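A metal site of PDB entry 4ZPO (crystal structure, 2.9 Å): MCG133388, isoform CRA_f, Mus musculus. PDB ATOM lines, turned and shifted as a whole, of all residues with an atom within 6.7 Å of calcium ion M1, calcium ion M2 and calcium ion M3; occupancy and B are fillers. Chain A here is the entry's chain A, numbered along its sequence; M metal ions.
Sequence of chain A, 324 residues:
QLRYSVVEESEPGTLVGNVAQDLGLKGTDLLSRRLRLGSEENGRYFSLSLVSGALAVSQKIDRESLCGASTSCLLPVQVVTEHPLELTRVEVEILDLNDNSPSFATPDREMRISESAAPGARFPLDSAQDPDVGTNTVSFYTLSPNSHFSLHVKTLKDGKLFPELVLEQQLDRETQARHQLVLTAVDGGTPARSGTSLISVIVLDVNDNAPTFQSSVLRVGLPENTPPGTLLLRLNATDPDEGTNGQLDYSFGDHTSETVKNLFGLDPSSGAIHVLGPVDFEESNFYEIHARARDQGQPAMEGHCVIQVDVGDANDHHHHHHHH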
ATOM      1  N   GLU A 115      24.579  -3.981  12.964  1.00  0.00           N
ATOM      2  CA  GLU A 115      24.985  -3.089  11.889  1.00  0.00           C
ATOM      3  C   GLU A 115      25.375  -1.715  12.444  1.00  0.00           C
ATOM      4  O   GLU A 115      26.059  -0.938  11.776  1.00  0.00           O
ATOM      5  CB  GLU A 115      23.862  -2.947  10.866  1.00  0.00           C
ATOM      6  CG  GLU A 115      24.249  -2.275   9.568  1.00  0.00           C
ATOM      7  CD  GLU A 115      23.087  -2.187   8.606  1.00  0.00           C
ATOM      8  OE1 GLU A 115      21.975  -2.615   8.970  1.00  0.00           O
ATOM      9  OE2 GLU A 115      23.292  -1.683   7.480  1.00  0.00           O
ATOM     10  N   GLN A 170      32.575   1.038   9.535  1.00  0.00           N
ATOM     11  CA  GLN A 170      31.205   0.664   9.881  1.00  0.00           C
ATOM     12  C   GLN A 170      30.651  -0.397   8.934  1.00  0.00           C
ATOM     13  O   GLN A 170      30.764  -0.270   7.713  1.00  0.00           O
ATOM     14  CB  GLN A 170      30.303   1.889   9.875  1.00  0.00           C
ATOM     15  CG  GLN A 170      28.839   1.592  10.169  1.00  0.00           C
ATOM     16  CD  GLN A 170      28.637   0.927  11.519  1.00  0.00           C
ATOM     17  OE1 GLN A 170      28.760  -0.295  11.646  1.00  0.00           O
ATOM     18  NE2 GLN A 170      28.326   1.722  12.533  1.00  0.00           N
ATOM     19  N   LEU A 171      30.043  -1.426   9.504  1.00  0.00           N
ATOM     20  CA  LEU A 171      29.444  -2.495   8.712  1.00  0.00           C
ATOM     21  C   LEU A 171      28.138  -2.024   8.074  1.00  0.00           C
ATOM     22  O   LEU A 171      27.467  -1.136   8.597  1.00  0.00           O
ATOM     23  CB  LEU A 171      29.178  -3.723   9.588  1.00  0.00           C
ATOM     24  CG  LEU A 171      30.378  -4.301  10.339  1.00  0.00           C
ATOM     25  CD1 LEU A 171      29.945  -5.448  11.232  1.00  0.00           C
ATOM     26  CD2 LEU A 171      31.456  -4.746   9.366  1.00  0.00           C
ATOM     27  N   ASP A 172      27.789  -2.621   6.940  1.00  0.00           N
ATOM     28  CA  ASP A 172      26.560  -2.274   6.242  1.00  0.00           C
ATOM     29  C   ASP A 172      25.910  -3.518   5.653  1.00  0.00           C
ATOM     30  O   ASP A 172      26.380  -4.074   4.659  1.00  0.00           O
ATOM     31  CB  ASP A 172      26.838  -1.253   5.143  1.00  0.00           C
ATOM     32  CG  ASP A 172      25.578  -0.778   4.448  1.00  0.00           C
ATOM     33  OD1 ASP A 172      24.499  -0.849   5.057  1.00  0.00           O
ATOM     34  OD2 ASP A 172      25.670  -0.323   3.279  1.00  0.00           O
ATOM     35  N   ARG A 173      24.805  -3.949   6.268  1.00  0.00           N
ATOM     36  CA  ARG A 173      24.102  -5.157   5.850  1.00  0.00           C
ATOM     37  C   ARG A 173      23.572  -5.048   4.428  1.00  0.00           C
ATOM     38  O   ARG A 173      23.434  -6.043   3.719  1.00  0.00           O
ATOM     39  CB  ARG A 173      22.943  -5.454   6.814  1.00  0.00           C
ATOM     40  CG  ARG A 173      22.205  -6.735   6.504  1.00  0.00           C
ATOM     41  CD  ARG A 173      20.808  -6.724   7.090  1.00  0.00           C
ATOM     42  NE  ARG A 173      19.869  -7.449   6.233  1.00  0.00           N
ATOM     43  CZ  ARG A 173      19.202  -6.897   5.232  1.00  0.00           C
ATOM     44  NH1 ARG A 173      19.359  -5.608   4.956  1.00  0.00           N
ATOM     45  NH2 ARG A 173      18.375  -7.627   4.496  1.00  0.00           N
ATOM     46  N   GLU A 174      23.284  -3.822   3.988  1.00  0.00           N
ATOM     47  CA  GLU A 174      22.742  -3.589   2.653  1.00  0.00           C
ATOM     48  C   GLU A 174      23.757  -3.890   1.552  1.00  0.00           C
ATOM     49  O   GLU A 174      23.385  -4.091   0.401  1.00  0.00           O
ATOM     50  CB  GLU A 174      22.231  -2.156   2.525  1.00  0.00           C
ATOM     51  CG  GLU A 174      20.841  -1.926   3.114  1.00  0.00           C
ATOM     52  CD  GLU A 174      20.819  -1.965   4.626  1.00  0.00           C
ATOM     53  OE1 GLU A 174      19.992  -2.701   5.192  1.00  0.00           O
ATOM     54  OE2 GLU A 174      21.629  -1.254   5.249  1.00  0.00           O
ATOM     55  N   LEU A 204      23.794  -8.198  11.768  1.00  0.00           N
ATOM     56  CA  LEU A 204      22.381  -8.068  12.127  1.00  0.00           C
ATOM     57  C   LEU A 204      21.827  -6.748  11.610  1.00  0.00           C
ATOM     58  O   LEU A 204      22.549  -5.751  11.539  1.00  0.00           O
ATOM     59  CB  LEU A 204      22.211  -8.154  13.647  1.00  0.00           C
ATOM     60  CG  LEU A 204      22.660  -9.460  14.294  1.00  0.00           C
ATOM     61  CD1 LEU A 204      22.492  -9.419  15.809  1.00  0.00           C
ATOM     62  CD2 LEU A 204      21.904 -10.645  13.703  1.00  0.00           C
ATOM     63  N   ASP A 205      20.557  -6.741  11.245  1.00  0.00           N
ATOM     64  CA  ASP A 205      19.948  -5.574  10.616  1.00  0.00           C
ATOM     65  C   ASP A 205      19.634  -4.454  11.603  1.00  0.00           C
ATOM     66  O   ASP A 205      19.213  -4.700  12.739  1.00  0.00           O
ATOM     67  CB  ASP A 205      18.673  -5.963   9.880  1.00  0.00           C
ATOM     68  CG  ASP A 205      18.109  -4.826   9.044  1.00  0.00           C
ATOM     69  OD1 ASP A 205      18.902  -4.107   8.410  1.00  0.00           O
ATOM     70  OD2 ASP A 205      16.864  -4.650   9.036  1.00  0.00           O
ATOM     71  N   VAL A 206      19.850  -3.222  11.159  1.00  0.00           N
ATOM     72  CA  VAL A 206      19.469  -2.033  11.911  1.00  0.00           C
ATOM     73  C   VAL A 206      18.763  -1.075  10.952  1.00  0.00           C
ATOM     74  O   VAL A 206      19.186  -0.928   9.810  1.00  0.00           O
ATOM     75  CB  VAL A 206      20.692  -1.335  12.549  1.00  0.00           C
ATOM     76  CG1 VAL A 206      20.311   0.031  13.110  1.00  0.00           C
ATOM     77  CG2 VAL A 206      21.305  -2.202  13.629  1.00  0.00           C
ATOM     78  N   ASN A 207      17.671  -0.459  11.405  1.00  0.00           N
ATOM     79  CA  ASN A 207      16.944   0.483  10.556  1.00  0.00           C
ATOM     80  C   ASN A 207      17.795   1.717  10.256  1.00  0.00           C
ATOM     81  O   ASN A 207      17.661   2.743  10.921  1.00  0.00           O
ATOM     82  CB  ASN A 207      15.627   0.891  11.210  1.00  0.00           C
ATOM     83  CG  ASN A 207      14.640   1.478  10.210  1.00  0.00           C
ATOM     84  OD1 ASN A 207      15.028   2.090   9.216  1.00  0.00           O
ATOM     85  ND2 ASN A 207      13.360   1.289  10.464  1.00  0.00           N
ATOM     86  N   ASP A 208      18.662   1.607   9.260  1.00  0.00           N
ATOM     87  CA  ASP A 208      19.525   2.717   8.873  1.00  0.00           C
ATOM     88  C   ASP A 208      19.206   3.190   7.454  1.00  0.00           C
ATOM     89  O   ASP A 208      20.055   3.758   6.775  1.00  0.00           O
ATOM     90  CB  ASP A 208      20.999   2.307   8.972  1.00  0.00           C
ATOM     91  CG  ASP A 208      21.390   1.255   7.947  1.00  0.00           C
ATOM     92  OD1 ASP A 208      21.145   0.058   8.195  1.00  0.00           O
ATOM     93  OD2 ASP A 208      21.947   1.629   6.891  1.00  0.00           O
ATOM     94  N   ASN A 209      17.978   2.939   7.021  1.00  0.00           N
ATOM     95  CA  ASN A 209      17.525   3.391   5.711  1.00  0.00           C
ATOM     96  C   ASN A 209      16.097   3.911   5.745  1.00  0.00           C
ATOM     97  O   ASN A 209      15.244   3.366   6.454  1.00  0.00           O
ATOM     98  CB  ASN A 209      17.648   2.266   4.691  1.00  0.00           C
ATOM     99  CG  ASN A 209      19.061   2.115   4.139  1.00  0.00           C
ATOM    100  OD1 ASN A 209      19.895   1.438   4.739  1.00  0.00           O
ATOM    101  ND2 ASN A 209      19.315   2.746   3.005  1.00  0.00           N
ATOM    102  N   ALA A 210      15.849   4.976   4.994  1.00  0.00           N
ATOM    103  CA  ALA A 210      14.514   5.539   4.890  1.00  0.00           C
ATOM    104  C   ALA A 210      13.896   5.179   3.552  1.00  0.00           C
ATOM    105  O   ALA A 210      14.607   5.078   2.547  1.00  0.00           O
ATOM    106  CB  ALA A 210      14.546   7.047   5.082  1.00  0.00           C
ATOM    107  N   PRO A 211      12.570   4.973   3.519  1.00  0.00           N
ATOM    108  CA  PRO A 211      11.867   4.695   2.262  1.00  0.00           C
ATOM    109  C   PRO A 211      12.100   5.805   1.238  1.00  0.00           C
ATOM    110  O   PRO A 211      12.210   6.965   1.616  1.00  0.00           O
ATOM    111  CB  PRO A 211      10.398   4.630   2.683  1.00  0.00           C
ATOM    112  CG  PRO A 211      10.444   4.240   4.119  1.00  0.00           C
ATOM    113  CD  PRO A 211      11.660   4.914   4.679  1.00  0.00           C
ATOM    114  N   ASP A 239      12.509   0.119   0.249  1.00  0.00           N
ATOM    115  CA  ASP A 239      13.276   0.147   1.479  1.00  0.00           C
ATOM    116  C   ASP A 239      14.144  -1.103   1.569  1.00  0.00           C
ATOM    117  O   ASP A 239      13.627  -2.223   1.641  1.00  0.00           O
ATOM    118  CB  ASP A 239      12.353   0.252   2.691  1.00  0.00           C
ATOM    119  CG  ASP A 239      13.082   0.692   3.940  1.00  0.00           C
ATOM    120  OD1 ASP A 239      13.794  -0.138   4.541  1.00  0.00           O
ATOM    121  OD2 ASP A 239      12.955   1.877   4.320  1.00  0.00           O
ATOM    122  N   PRO A 240      15.471  -0.927   1.560  1.00  0.00           N
ATOM    123  CA  PRO A 240      16.445  -2.028   1.502  1.00  0.00           C
ATOM    124  C   PRO A 240      16.609  -2.779   2.829  1.00  0.00           C
ATOM    125  O   PRO A 240      17.283  -3.808   2.853  1.00  0.00           O
ATOM    126  CB  PRO A 240      17.735  -1.322   1.110  1.00  0.00           C
ATOM    127  CG  PRO A 240      17.603   0.041   1.695  1.00  0.00           C
ATOM    128  CD  PRO A 240      16.135   0.393   1.580  1.00  0.00           C
ATOM    129  N   ASP A 241      16.031  -2.260   3.901  1.00  0.00           N
ATOM    130  CA  ASP A 241      16.191  -2.877   5.220  1.00  0.00           C
ATOM    131  C   ASP A 241      15.410  -4.183   5.325  1.00  0.00           C
ATOM    132  O   ASP A 241      14.516  -4.461   4.530  1.00  0.00           O
ATOM    133  CB  ASP A 241      15.757  -1.906   6.317  1.00  0.00           C
ATOM    134  CG  ASP A 241      16.693  -0.728   6.452  1.00  0.00           C
ATOM    135  OD1 ASP A 241      17.871  -0.848   6.053  1.00  0.00           O
ATOM    136  OD2 ASP A 241      16.265   0.326   6.977  1.00  0.00           O
ATOM    137  N   GLU A 242      15.773  -4.985   6.324  1.00  0.00           N
ATOM    138  CA  GLU A 242      15.219  -6.328   6.489  1.00  0.00           C
ATOM    139  C   GLU A 242      13.983  -6.358   7.378  1.00  0.00           C
ATOM    140  O   GLU A 242      13.905  -5.638   8.380  1.00  0.00           O
ATOM    141  CB  GLU A 242      16.290  -7.265   7.065  1.00  0.00           C
ATOM    142  CG  GLU A 242      15.858  -8.709   7.228  1.00  0.00           C
ATOM    143  CD  GLU A 242      16.939  -9.567   7.837  1.00  0.00           C
ATOM    144  OE1 GLU A 242      18.004  -9.026   8.203  1.00  0.00           O
ATOM    145  OE2 GLU A 242      16.729 -10.797   7.961  1.00  0.00           O
ATOM    146  N   THR A 244      10.458  -5.925   9.146  1.00  0.00           N
ATOM    147  CA  THR A 244       9.568  -4.797   9.397  1.00  0.00           C
ATOM    148  C   THR A 244      10.267  -3.467   9.119  1.00  0.00           C
ATOM    149  O   THR A 244       9.616  -2.470   8.825  1.00  0.00           O
ATOM    150  CB  THR A 244       9.052  -4.802  10.851  1.00  0.00           C
ATOM    151  OG1 THR A 244      10.163  -4.707  11.751  1.00  0.00           O
ATOM    152  CG2 THR A 244       8.278  -6.073  11.129  1.00  0.00           C
ATOM    153  N   ASN A 245      11.588  -3.472   9.202  1.00  0.00           N
ATOM    154  CA  ASN A 245      12.375  -2.287   8.890  1.00  0.00           C
ATOM    155  C   ASN A 245      12.317  -1.955   7.409  1.00  0.00           C
ATOM    156  O   ASN A 245      12.640  -0.837   7.001  1.00  0.00           O
ATOM    157  CB  ASN A 245      13.826  -2.478   9.335  1.00  0.00           C
ATOM    158  CG  ASN A 245      13.991  -2.535  10.835  1.00  0.00           C
ATOM    159  OD1 ASN A 245      13.007  -2.667  11.570  1.00  0.00           O
ATOM    160  ND2 ASN A 245      15.225  -2.446  11.311  1.00  0.00           N
ATOM    161  N   GLY A 246      11.900  -2.921   6.598  1.00  0.00           N
ATOM    162  CA  GLY A 246      11.808  -2.742   5.164  1.00  0.00           C
ATOM    163  C   GLY A 246      10.397  -2.526   4.658  1.00  0.00           C
ATOM    164  O   GLY A 246      10.190  -1.998   3.571  1.00  0.00           O
ATOM    165  N   GLN A 247       9.412  -2.945   5.449  1.00  0.00           N
ATOM    166  CA  GLN A 247       8.011  -2.759   5.088  1.00  0.00           C
ATOM    167  C   GLN A 247       7.564  -1.331   5.395  1.00  0.00           C
ATOM    168  O   GLN A 247       8.023  -0.728   6.368  1.00  0.00           O
ATOM    169  CB  GLN A 247       7.120  -3.770   5.815  1.00  0.00           C
ATOM    170  CG  GLN A 247       7.266  -5.195   5.291  1.00  0.00           C
ATOM    171  CD  GLN A 247       6.285  -6.151   5.937  1.00  0.00           C
ATOM    172  OE1 GLN A 247       6.193  -6.243   7.164  1.00  0.00           O
ATOM    173  NE2 GLN A 247       5.532  -6.864   5.110  1.00  0.00           N
ATOM    174  N   ASP A 295       7.963   4.090   7.567  1.00  0.00           N
ATOM    175  CA  ASP A 295       8.585   2.804   7.873  1.00  0.00           C
ATOM    176  C   ASP A 295       7.863   2.118   9.018  1.00  0.00           C
ATOM    177  O   ASP A 295       6.964   2.695   9.636  1.00  0.00           O
ATOM    178  CB  ASP A 295      10.063   2.991   8.215  1.00  0.00           C
ATOM    179  CG  ASP A 295      10.900   1.795   7.848  1.00  0.00           C
ATOM    180  OD1 ASP A 295      10.326   0.750   7.506  1.00  0.00           O
ATOM    181  OD2 ASP A 295      12.146   1.904   7.929  1.00  0.00           O
ATOM    182  N   GLN A 296       8.247   0.877   9.313  1.00  0.00           N
ATOM    183  CA  GLN A 296       7.652   0.138  10.424  1.00  0.00           C
ATOM    184  C   GLN A 296       8.704  -0.264  11.453  1.00  0.00           C
ATOM    185  O   GLN A 296       8.444  -1.089  12.335  1.00  0.00           O
ATOM    186  CB  GLN A 296       6.926  -1.102   9.913  1.00  0.00           C
ATOM    187  CG  GLN A 296       5.659  -0.806   9.137  1.00  0.00           C
ATOM    188  CD  GLN A 296       4.858  -2.057   8.833  1.00  0.00           C
ATOM    189  OE1 GLN A 296       5.198  -3.150   9.277  1.00  0.00           O
ATOM    190  NE2 GLN A 296       3.775  -1.899   8.073  1.00  0.00           N
ATOM    191  N   GLY A 297       9.888   0.320  11.347  1.00  0.00           N
ATOM    192  CA  GLY A 297      10.962   0.028  12.283  1.00  0.00           C
ATOM    193  C   GLY A 297      10.984   0.993  13.454  1.00  0.00           C
ATOM    194  O   GLY A 297      10.209   1.936  13.512  1.00  0.00           O
ATOM    195  N   MET A 301      11.399   5.477   9.935  1.00  0.00           N
ATOM    196  CA  MET A 301      11.936   6.348   8.891  1.00  0.00           C
ATOM    197  C   MET A 301      10.836   6.688   7.889  1.00  0.00           C
ATOM    198  O   MET A 301       9.782   6.047   7.877  1.00  0.00           O
ATOM    199  CB  MET A 301      13.108   5.670   8.181  1.00  0.00           C
ATOM    200  CG  MET A 301      14.250   5.248   9.096  1.00  0.00           C
ATOM    201  SD  MET A 301      15.050   6.640   9.921  1.00  0.00           S
ATOM    202  CE  MET A 301      16.594   5.891  10.418  1.00  0.00           C
HETATM  203 CA    CA M   1      14.023   1.262   6.593  1.00  0.00          CA
HETATM  204 CA    CA M   2      19.777  -1.931   7.592  1.00  0.00          CA
HETATM  205 CA    CA M   3      24.151   0.600   7.028  1.00  0.00          CA
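Calcium ion M2 is bound by the side-chain carboxylate (OD1) of Asp 205 (2.5 Å).
Calcium ion M2 is bound by the side-chain carboxylate (OD1) of Asp 208 (2.5 Å).
Calcium ion M2 is bound by the backbone carbonyl oxygen (O) of Val 206, 2.5 Å away.
The side-chain carboxylate (OE1) of Glu 174 is bound to calcium ion M2.
Calcium ion M2 is bound by OD1 of Asp 241 (2.7 Å).
OE1 of Glu 115 is bound to calcium ion M2.
Calcium ion M2 has six donor atoms within binding distance.
Slightly farther from calcium ion M2 lies the side-chain carboxylate (OE2) of Glu 174 (3.1 Å).
Along chain A the residues within 4 Å of calcium ion M3 span positions 115 to 208.
The nearest printed residue that does not touch calcium ion M3 is Leu 171 (4.1 Å).
Within 4 Å of calcium ion M2: Glu 115, Glu 174, Asp 205, Val 206, Asp 208 and Asp 241.
The side-chain carboxylate (OD2) of Asp 208 is bound to calcium ion M3 (2.4 Å).
Calcium ion M3 is bound by OD1 of Asp 172, 2.5 Å away.
OE2 of Glu 115 is bound to calcium ion M3.
Calcium ion M3 has three donor atoms within binding distance.
Calcium ion M1 is bound by the side-chain carboxylate (OD2) of Asp 295 (2.4 Å), the backbone carbonyl oxygen (O) of Asn 209 (2.4 Å), the side-chain carboxylate (OD2) of Asp 241 (2.5 Å), the side-chain carboxylate (OD1) of Asp 239 (2.5 Å), the backbone carbonyl oxygen (O) of Asn 245 (2.5 Å) and the side-chain carboxylate (OD2) of Asp 239 (2.6 Å).
Slightly farther from calcium ion M1 lies the side-chain amide oxygen (OD1) of Asn 207 (2.9 Å).
Within 4 Å of calcium ion M1: Asn 207, Asn 209, Asp 239, Asp 241, Asn 245 and Asp 295.
The nearest printed residue that does not touch calcium ion M1 is Ala 210 (4.4 Å).
N of Asp 295 sits at hydrogen-bond distance from O of Met 301 (2.7 Å).
The side-chain carboxylate (OD2) of Asp 208 sits close to the side-chain amide oxygen (OD1) of Asn 209, 3.0 Å away.
O of Asn 209 sits close to OD1 of Asn 207.
OD1 of Asn 207 lies close to OD2 of Asp 241 (3.1 Å).
The backbone carbonyl oxygen (O) of Leu 204 is in hydrogen-bond range of the backbone NH (N) of Glu 115, at 3.0 Å.
NH1 of Arg 173 lies close to OD1 of Asp 205, at 3.8 Å.
N of Glu 242 is in hydrogen-bond range of OD2 of Asp 205 (2.9 Å).
The side-chain carboxylate of Glu 174 sits close to the guanidinium group of Arg 173 (3.0 Å).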
